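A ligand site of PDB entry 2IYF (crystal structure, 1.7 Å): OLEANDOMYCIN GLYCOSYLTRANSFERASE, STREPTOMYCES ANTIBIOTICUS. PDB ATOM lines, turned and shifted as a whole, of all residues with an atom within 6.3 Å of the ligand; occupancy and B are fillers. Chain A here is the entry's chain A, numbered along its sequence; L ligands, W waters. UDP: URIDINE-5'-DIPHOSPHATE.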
ATOM      1  N   SER A 238       2.114  21.669 -18.321  1.00  0.00           N
ATOM      2  CA  SER A 238       3.180  22.343 -17.596  1.00  0.00           C
ATOM      3  C   SER A 238       3.749  23.459 -18.487  1.00  0.00           C
ATOM      4  O   SER A 238       4.250  23.208 -19.569  1.00  0.00           O
ATOM      5  CB  SER A 238       4.282  21.343 -17.199  1.00  0.00           C
ATOM      6  OG  SER A 238       5.379  22.012 -16.635  1.00  0.00           O
ATOM      7  N   LEU A 239       3.647  24.694 -18.016  1.00  0.00           N
ATOM      8  CA  LEU A 239       4.208  25.814 -18.780  1.00  0.00           C
ATOM      9  C   LEU A 239       5.621  26.205 -18.305  1.00  0.00           C
ATOM     10  O   LEU A 239       6.040  27.350 -18.498  1.00  0.00           O
ATOM     11  CB  LEU A 239       3.251  27.018 -18.764  1.00  0.00           C
ATOM     12  CG  LEU A 239       1.848  26.832 -19.352  1.00  0.00           C
ATOM     13  CD1 LEU A 239       1.095  28.167 -19.332  1.00  0.00           C
ATOM     14  CD2 LEU A 239       1.812  26.182 -20.773  1.00  0.00           C
ATOM     15  N   GLY A 240       6.326  25.249 -17.714  1.00  0.00           N
ATOM     16  CA  GLY A 240       7.711  25.428 -17.271  1.00  0.00           C
ATOM     17  C   GLY A 240       7.782  25.951 -15.847  1.00  0.00           C
ATOM     18  O   GLY A 240       6.934  25.645 -15.014  1.00  0.00           O
ATOM     19  N   SER A 241       8.818  26.762 -15.594  1.00  0.00           N
ATOM     20  CA  SER A 241       9.115  27.269 -14.245  1.00  0.00           C
ATOM     21  C   SER A 241       8.911  28.774 -14.082  1.00  0.00           C
ATOM     22  O   SER A 241       9.015  29.285 -12.975  1.00  0.00           O
ATOM     23  CB  SER A 241      10.556  26.908 -13.846  1.00  0.00           C
ATOM     24  OG  SER A 241      10.707  25.507 -13.632  1.00  0.00           O
ATOM     25  N   ALA A 242       8.628  29.475 -15.177  1.00  0.00           N
ATOM     26  CA  ALA A 242       8.525  30.939 -15.117  1.00  0.00           C
ATOM     27  C   ALA A 242       7.199  31.519 -15.642  1.00  0.00           C
ATOM     28  O   ALA A 242       6.535  32.286 -14.945  1.00  0.00           O
ATOM     29  CB  ALA A 242       9.734  31.584 -15.831  1.00  0.00           C
ATOM     30  N   PHE A 243       6.803  31.137 -16.859  1.00  0.00           N
ATOM     31  CA  PHE A 243       5.616  31.707 -17.506  1.00  0.00           C
ATOM     32  C   PHE A 243       4.326  30.964 -17.148  1.00  0.00           C
ATOM     33  O   PHE A 243       3.531  30.617 -18.024  1.00  0.00           O
ATOM     34  N   GLN A 268       0.203  21.146 -13.715  1.00  0.00           N
ATOM     35  CA  GLN A 268       1.286  21.779 -12.964  1.00  0.00           C
ATOM     36  C   GLN A 268       1.032  23.283 -13.042  1.00  0.00           C
ATOM     37  O   GLN A 268       1.127  23.866 -14.107  1.00  0.00           O
ATOM     38  CB  GLN A 268       2.646  21.389 -13.546  1.00  0.00           C
ATOM     39  CG  GLN A 268       3.843  21.814 -12.711  1.00  0.00           C
ATOM     40  CD  GLN A 268       4.301  23.238 -13.018  1.00  0.00           C
ATOM     41  OE1 GLN A 268       4.240  24.108 -12.152  1.00  0.00           O
ATOM     42  NE2 GLN A 268       4.732  23.484 -14.256  1.00  0.00           N
ATOM     43  N   ASP A 289       1.838  22.200  -7.495  1.00  0.00           N
ATOM     44  CA  ASP A 289       2.578  23.441  -7.776  1.00  0.00           C
ATOM     45  C   ASP A 289       3.894  23.143  -8.478  1.00  0.00           C
ATOM     46  O   ASP A 289       4.438  23.992  -9.166  1.00  0.00           O
ATOM     47  CB  ASP A 289       2.788  24.268  -6.498  1.00  0.00           C
ATOM     48  CG  ASP A 289       3.620  23.545  -5.451  1.00  0.00           C
ATOM     49  OD1 ASP A 289       3.756  22.292  -5.485  1.00  0.00           O
ATOM     50  OD2 ASP A 289       4.161  24.263  -4.573  1.00  0.00           O
ATOM     51  N   TRP A 290       4.373  21.918  -8.306  1.00  0.00           N
ATOM     52  CA  TRP A 290       5.573  21.436  -8.949  1.00  0.00           C
ATOM     53  C   TRP A 290       5.440  19.928  -9.149  1.00  0.00           C
ATOM     54  O   TRP A 290       4.864  19.226  -8.308  1.00  0.00           O
ATOM     55  CB  TRP A 290       6.822  21.796  -8.103  1.00  0.00           C
ATOM     56  CG  TRP A 290       8.094  21.186  -8.618  1.00  0.00           C
ATOM     57  CD1 TRP A 290       9.018  21.776  -9.429  1.00  0.00           C
ATOM     58  CD2 TRP A 290       8.575  19.847  -8.380  1.00  0.00           C
ATOM     59  NE1 TRP A 290      10.046  20.907  -9.711  1.00  0.00           N
ATOM     60  CE2 TRP A 290       9.792  19.705  -9.095  1.00  0.00           C
ATOM     61  CE3 TRP A 290       8.084  18.758  -7.649  1.00  0.00           C
ATOM     62  CZ2 TRP A 290      10.522  18.520  -9.077  1.00  0.00           C
ATOM     63  CZ3 TRP A 290       8.820  17.571  -7.638  1.00  0.00           C
ATOM     64  CH2 TRP A 290      10.019  17.469  -8.355  1.00  0.00           C
ATOM     65  N   VAL A 291       5.945  19.419 -10.276  1.00  0.00           N
ATOM     66  CA  VAL A 291       5.975  17.979 -10.538  1.00  0.00           C
ATOM     67  C   VAL A 291       7.343  17.450 -10.947  1.00  0.00           C
ATOM     68  O   VAL A 291       8.154  18.211 -11.479  1.00  0.00           O
ATOM     69  CB  VAL A 291       4.938  17.581 -11.637  1.00  0.00           C
ATOM     70  CG1 VAL A 291       3.551  18.017 -11.227  1.00  0.00           C
ATOM     71  CG2 VAL A 291       5.321  18.187 -13.021  1.00  0.00           C
ATOM     72  N   PRO A 292       7.595  16.142 -10.720  1.00  0.00           N
ATOM     73  CA  PRO A 292       8.764  15.523 -11.330  1.00  0.00           C
ATOM     74  C   PRO A 292       8.464  15.333 -12.840  1.00  0.00           C
ATOM     75  O   PRO A 292       7.958  14.281 -13.258  1.00  0.00           O
ATOM     76  CB  PRO A 292       8.915  14.207 -10.569  1.00  0.00           C
ATOM     77  CG  PRO A 292       7.545  13.907 -10.035  1.00  0.00           C
ATOM     78  CD  PRO A 292       6.819  15.198  -9.884  1.00  0.00           C
ATOM     79  N   GLN A 293       8.750  16.373 -13.618  1.00  0.00           N
ATOM     80  CA  GLN A 293       8.242  16.483 -14.984  1.00  0.00           C
ATOM     81  C   GLN A 293       8.725  15.369 -15.889  1.00  0.00           C
ATOM     82  O   GLN A 293       7.946  14.755 -16.623  1.00  0.00           O
ATOM     83  CB  GLN A 293       8.577  17.833 -15.582  1.00  0.00           C
ATOM     84  CG  GLN A 293       8.160  17.962 -17.040  1.00  0.00           C
ATOM     85  CD  GLN A 293       8.082  19.389 -17.483  1.00  0.00           C
ATOM     86  OE1 GLN A 293       7.336  20.203 -16.936  1.00  0.00           O
ATOM     87  NE2 GLN A 293       8.798  19.685 -18.542  1.00  0.00           N
ATOM     88  N   LEU A 294      10.023  15.104 -15.840  1.00  0.00           N
ATOM     89  CA  LEU A 294      10.582  14.034 -16.658  1.00  0.00           C
ATOM     90  C   LEU A 294       9.963  12.698 -16.272  1.00  0.00           C
ATOM     91  O   LEU A 294       9.633  11.896 -17.149  1.00  0.00           O
ATOM     92  CB  LEU A 294      12.098  13.999 -16.545  1.00  0.00           C
ATOM     93  CG  LEU A 294      12.820  13.039 -17.478  1.00  0.00           C
ATOM     94  CD1 LEU A 294      12.549  13.367 -18.975  1.00  0.00           C
ATOM     95  CD2 LEU A 294      14.320  13.041 -17.191  1.00  0.00           C
ATOM     96  N   LEU A 297       6.494  12.588 -17.748  1.00  0.00           N
ATOM     97  CA  LEU A 297       6.548  12.477 -19.206  1.00  0.00           C
ATOM     98  C   LEU A 297       6.890  11.065 -19.647  1.00  0.00           C
ATOM     99  O   LEU A 297       6.412  10.631 -20.661  1.00  0.00           O
ATOM    100  CB  LEU A 297       7.537  13.480 -19.818  1.00  0.00           C
ATOM    101  CG  LEU A 297       7.042  14.944 -19.815  1.00  0.00           C
ATOM    102  CD1 LEU A 297       8.146  15.915 -20.282  1.00  0.00           C
ATOM    103  CD2 LEU A 297       5.825  15.111 -20.701  1.00  0.00           C
ATOM    104  N   THR A 305       2.526  21.955 -23.469  1.00  0.00           N
ATOM    105  CA  THR A 305       3.798  22.646 -23.089  1.00  0.00           C
ATOM    106  C   THR A 305       3.834  24.087 -23.617  1.00  0.00           C
ATOM    107  O   THR A 305       3.262  24.374 -24.666  1.00  0.00           O
ATOM    108  CB  THR A 305       5.033  21.862 -23.670  1.00  0.00           C
ATOM    109  OG1 THR A 305       6.260  22.521 -23.317  1.00  0.00           O
ATOM    110  CG2 THR A 305       4.946  21.651 -25.212  1.00  0.00           C
ATOM    111  N   HIS A 306       4.506  25.011 -22.899  1.00  0.00           N
ATOM    112  CA  HIS A 306       4.808  26.328 -23.460  1.00  0.00           C
ATOM    113  C   HIS A 306       5.926  26.277 -24.528  1.00  0.00           C
ATOM    114  O   HIS A 306       6.202  27.290 -25.171  1.00  0.00           O
ATOM    115  CB  HIS A 306       5.166  27.329 -22.345  1.00  0.00           C
ATOM    116  CG  HIS A 306       6.518  27.082 -21.722  1.00  0.00           C
ATOM    117  ND1 HIS A 306       6.983  25.825 -21.404  1.00  0.00           N
ATOM    118  CD2 HIS A 306       7.484  27.957 -21.334  1.00  0.00           C
ATOM    119  CE1 HIS A 306       8.184  25.928 -20.861  1.00  0.00           C
ATOM    120  NE2 HIS A 306       8.500  27.208 -20.783  1.00  0.00           N
ATOM    121  N   ALA A 307       6.498  25.104 -24.751  1.00  0.00           N
ATOM    122  CA  ALA A 307       7.574  24.928 -25.758  1.00  0.00           C
ATOM    123  C   ALA A 307       8.872  25.662 -25.371  1.00  0.00           C
ATOM    124  O   ALA A 307       9.647  26.093 -26.266  1.00  0.00           O
ATOM    125  CB  ALA A 307       7.103  25.352 -27.144  1.00  0.00           C
ATOM    126  N   GLY A 308       9.133  25.828 -24.059  1.00  0.00           N
ATOM    127  CA  GLY A 308      10.483  26.197 -23.629  1.00  0.00           C
ATOM    128  C   GLY A 308      11.529  25.180 -24.062  1.00  0.00           C
ATOM    129  O   GLY A 308      11.204  24.047 -24.437  1.00  0.00           O
ATOM    130  N   ALA A 309      12.815  25.538 -24.001  1.00  0.00           N
ATOM    131  CA  ALA A 309      13.862  24.608 -24.462  1.00  0.00           C
ATOM    132  C   ALA A 309      13.843  23.235 -23.756  1.00  0.00           C
ATOM    133  O   ALA A 309      13.972  22.177 -24.383  1.00  0.00           O
ATOM    134  CB  ALA A 309      15.246  25.254 -24.336  1.00  0.00           C
ATOM    135  N   GLY A 310      13.695  23.265 -22.429  1.00  0.00           N
ATOM    136  CA  GLY A 310      13.686  22.045 -21.617  1.00  0.00           C
ATOM    137  C   GLY A 310      12.475  21.197 -21.949  1.00  0.00           C
ATOM    138  O   GLY A 310      12.601  20.023 -22.326  1.00  0.00           O
ATOM    139  N   GLY A 311      11.293  21.779 -21.806  1.00  0.00           N
ATOM    140  CA  GLY A 311      10.050  21.037 -22.091  1.00  0.00           C
ATOM    141  C   GLY A 311      10.028  20.449 -23.481  1.00  0.00           C
ATOM    142  O   GLY A 311       9.653  19.290 -23.661  1.00  0.00           O
ATOM    143  N   SER A 312      10.514  21.210 -24.469  1.00  0.00           N
ATOM    144  CA  SER A 312      10.481  20.770 -25.877  1.00  0.00           C
ATOM    145  C   SER A 312      11.407  19.555 -25.995  1.00  0.00           C
ATOM    146  O   SER A 312      11.000  18.519 -26.536  1.00  0.00           O
ATOM    147  CB  SER A 312      10.912  21.901 -26.846  1.00  0.00           C
ATOM    148  OG  SER A 312      10.031  23.044 -26.800  1.00  0.00           O
ATOM    149  N   GLU A 314      12.428  17.505 -23.643  1.00  0.00           N
ATOM    150  CA  GLU A 314      11.941  16.393 -22.821  1.00  0.00           C
ATOM    151  C   GLU A 314      10.772  15.676 -23.456  1.00  0.00           C
ATOM    152  O   GLU A 314      10.652  14.458 -23.366  1.00  0.00           O
ATOM    153  CB  GLU A 314      11.527  16.914 -21.448  1.00  0.00           C
ATOM    154  CG  GLU A 314      12.749  17.272 -20.597  1.00  0.00           C
ATOM    155  CD  GLU A 314      12.464  18.225 -19.475  1.00  0.00           C
ATOM    156  OE1 GLU A 314      11.278  18.469 -19.144  1.00  0.00           O
ATOM    157  OE2 GLU A 314      13.480  18.713 -18.905  1.00  0.00           O
ATOM    158  N   ASP A 330      11.075  33.540 -26.748  1.00  0.00           N
ATOM    159  CA  ASP A 330      11.949  32.387 -26.836  1.00  0.00           C
ATOM    160  C   ASP A 330      11.259  31.023 -27.129  1.00  0.00           C
ATOM    161  O   ASP A 330      11.946  30.005 -27.215  1.00  0.00           O
ATOM    162  CB  ASP A 330      12.807  32.296 -25.562  1.00  0.00           C
ATOM    163  CG  ASP A 330      12.118  32.917 -24.342  1.00  0.00           C
ATOM    164  OD1 ASP A 330      11.090  32.366 -23.898  1.00  0.00           O
ATOM    165  OD2 ASP A 330      12.625  33.946 -23.809  1.00  0.00           O
ATOM    166  N   GLN A 331       9.922  31.007 -27.277  1.00  0.00           N
ATOM    167  CA  GLN A 331       9.178  29.739 -27.445  1.00  0.00           C
ATOM    168  C   GLN A 331       8.469  29.544 -28.783  1.00  0.00           C
ATOM    169  O   GLN A 331       8.118  28.416 -29.141  1.00  0.00           O
ATOM    170  CB  GLN A 331       8.146  29.605 -26.326  1.00  0.00           C
ATOM    171  CG  GLN A 331       8.751  29.337 -24.948  1.00  0.00           C
ATOM    172  CD  GLN A 331       8.144  30.202 -23.861  1.00  0.00           C
ATOM    173  OE1 GLN A 331       6.938  30.474 -23.836  1.00  0.00           O
ATOM    174  NE2 GLN A 331       8.987  30.648 -22.938  1.00  0.00           N
HETATM  175  N1  UDP L   1      10.284  21.428 -14.399  1.00  0.00           N
HETATM  176  C2  UDP L   1       9.991  20.380 -13.544  1.00  0.00           C
HETATM  177  N3  UDP L   1       8.823  20.418 -12.808  1.00  0.00           N
HETATM  178  C4  UDP L   1       7.969  21.502 -12.894  1.00  0.00           C
HETATM  179  C5  UDP L   1       8.278  22.558 -13.739  1.00  0.00           C
HETATM  180  C6  UDP L   1       9.360  22.434 -14.597  1.00  0.00           C
HETATM  181  O2  UDP L   1      10.722  19.393 -13.444  1.00  0.00           O
HETATM  182  O4  UDP L   1       6.939  21.517 -12.211  1.00  0.00           O
HETATM  183  C1' UDP L   1      11.532  21.395 -15.204  1.00  0.00           C
HETATM  184  C2' UDP L   1      11.263  20.918 -16.620  1.00  0.00           C
HETATM  185  O2' UDP L   1      11.313  19.510 -16.661  1.00  0.00           O
HETATM  186  C3' UDP L   1      12.361  21.605 -17.413  1.00  0.00           C
HETATM  187  C4' UDP L   1      12.539  22.917 -16.657  1.00  0.00           C
HETATM  188  O4' UDP L   1      12.037  22.716 -15.345  1.00  0.00           O
HETATM  189  O3' UDP L   1      13.563  20.861 -17.365  1.00  0.00           O
HETATM  190  C5' UDP L   1      11.768  24.058 -17.309  1.00  0.00           C
HETATM  191  O5' UDP L   1      12.566  24.505 -18.390  1.00  0.00           O
HETATM  192  PA  UDP L   1      11.920  25.080 -19.744  1.00  0.00           P
HETATM  193  O1A UDP L   1      13.017  25.493 -20.661  1.00  0.00           O
HETATM  194  O2A UDP L   1      11.025  24.059 -20.346  1.00  0.00           O
HETATM  195  O3A UDP L   1      10.952  26.297 -19.327  1.00  0.00           O
HETATM  196  PB  UDP L   1      11.318  27.722 -18.666  1.00  0.00           P
HETATM  197  O1B UDP L   1      10.951  27.621 -17.223  1.00  0.00           O
HETATM  198  O2B UDP L   1      10.474  28.711 -19.369  1.00  0.00           O
HETATM  199  O3B UDP L   1      12.758  28.036 -18.826  1.00  0.00           O
HETATM  200  O   HOH W   1      15.140  20.135 -14.980  1.00  0.00           O
HETATM  201  O   HOH W   2      15.066  26.717 -18.062  1.00  0.00           O
HETATM  202  O   HOH W   3      15.981  22.300 -18.509  1.00  0.00           O
HETATM  203  O   HOH W   4       8.783  22.721 -19.131  1.00  0.00           O
HETATM  204  O   HOH W   5      12.099  17.069 -14.442  1.00  0.00           O
HETATM  205  O   HOH W   6      14.017  17.521 -16.340  1.00  0.00           O
HETATM  206  O   HOH W   7       7.984  29.057 -17.886  1.00  0.00           O
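The side-chain carboxylate (OE2) of Glu 314 sits at hydrogen-bond distance from an oxygen (O3') of the ligand (2.6 Å). The backbone NH of Val 291 is in hydrogen-bond range of an oxygen (O4) of the ligand, at 3.0 Å. The backbone carbonyl oxygen (O) of Val 291 is in hydrogen-bond range of a nitrogen (N3) of the ligand, at 2.7 Å. The backbone NH (N) of Gly 311 lies within hydrogen-bond range of an oxygen (O2A) of the ligand (2.7 Å). The backbone NH (N) of Ser 241 is in hydrogen-bond range of an oxygen (O1B) of the ligand (2.8 Å). O2B of the ligand lies within hydrogen-bond range of NE2 of His 306 (2.9 Å). The backbone NH (N) of Gly 310 is in hydrogen-bond range of an oxygen (O1A) of the ligand (2.9 Å). The side-chain amide nitrogen (NE2) of Gln 293 lies within hydrogen-bond range of an oxygen (O2') of the ligand, 3.1 Å away. An oxygen (O1A) of the ligand lies within hydrogen-bond range of the backbone NH (N) of Ala 309 (3.3 Å).
OE1 of Glu 314 lies within hydrogen-bond range of NE2 of Gln 293. N of Gly 308 lies close to ND1 of His 306, at 3.4 Å. A ring nitrogen (NE2) of His 306 sits close to the backbone carbonyl oxygen (O) of Leu 239 (3.4 Å). OE1 of Gln 293 sits at hydrogen-bond distance from OG of Ser 238 (2.7 Å). NE2 of Gln 268 is in hydrogen-bond range of O of Gly 240, 3.2 Å away. NE2 of Gln 268 lies within hydrogen-bond range of OG of Ser 238 (2.9 Å). O of Asp 289 lies close to OE1 of Gln 268. O of Gly 308 lies within hydrogen-bond range of OG of Ser 312 (2.8 Å).
A nitrogen (N3) of the ligand sits close to the indole nitrogen (NE1) of Trp 290, at 3.4 Å. Merely in contact with the ligand: Gly 240, Ala 242, Gln 268 and Gly 308. Of the 25 residues printed, 13 come within 4 Å of the ligand. Along chain A the residues within 4 Å of the ligand span positions 240 to 314.
Water W5 bridges an oxygen (O2) of the ligand (2.9 Å) and the backbone NH (N) of Leu 294 (3.2 Å). Water W4 bridges an oxygen (O2A) of the ligand (2.9 Å) and the side-chain amide nitrogen of Gln 293 (3.1 Å). Water W6 bridges OE2 of Glu 314 (2.9 Å) and O2' of the ligand (3.4 Å).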
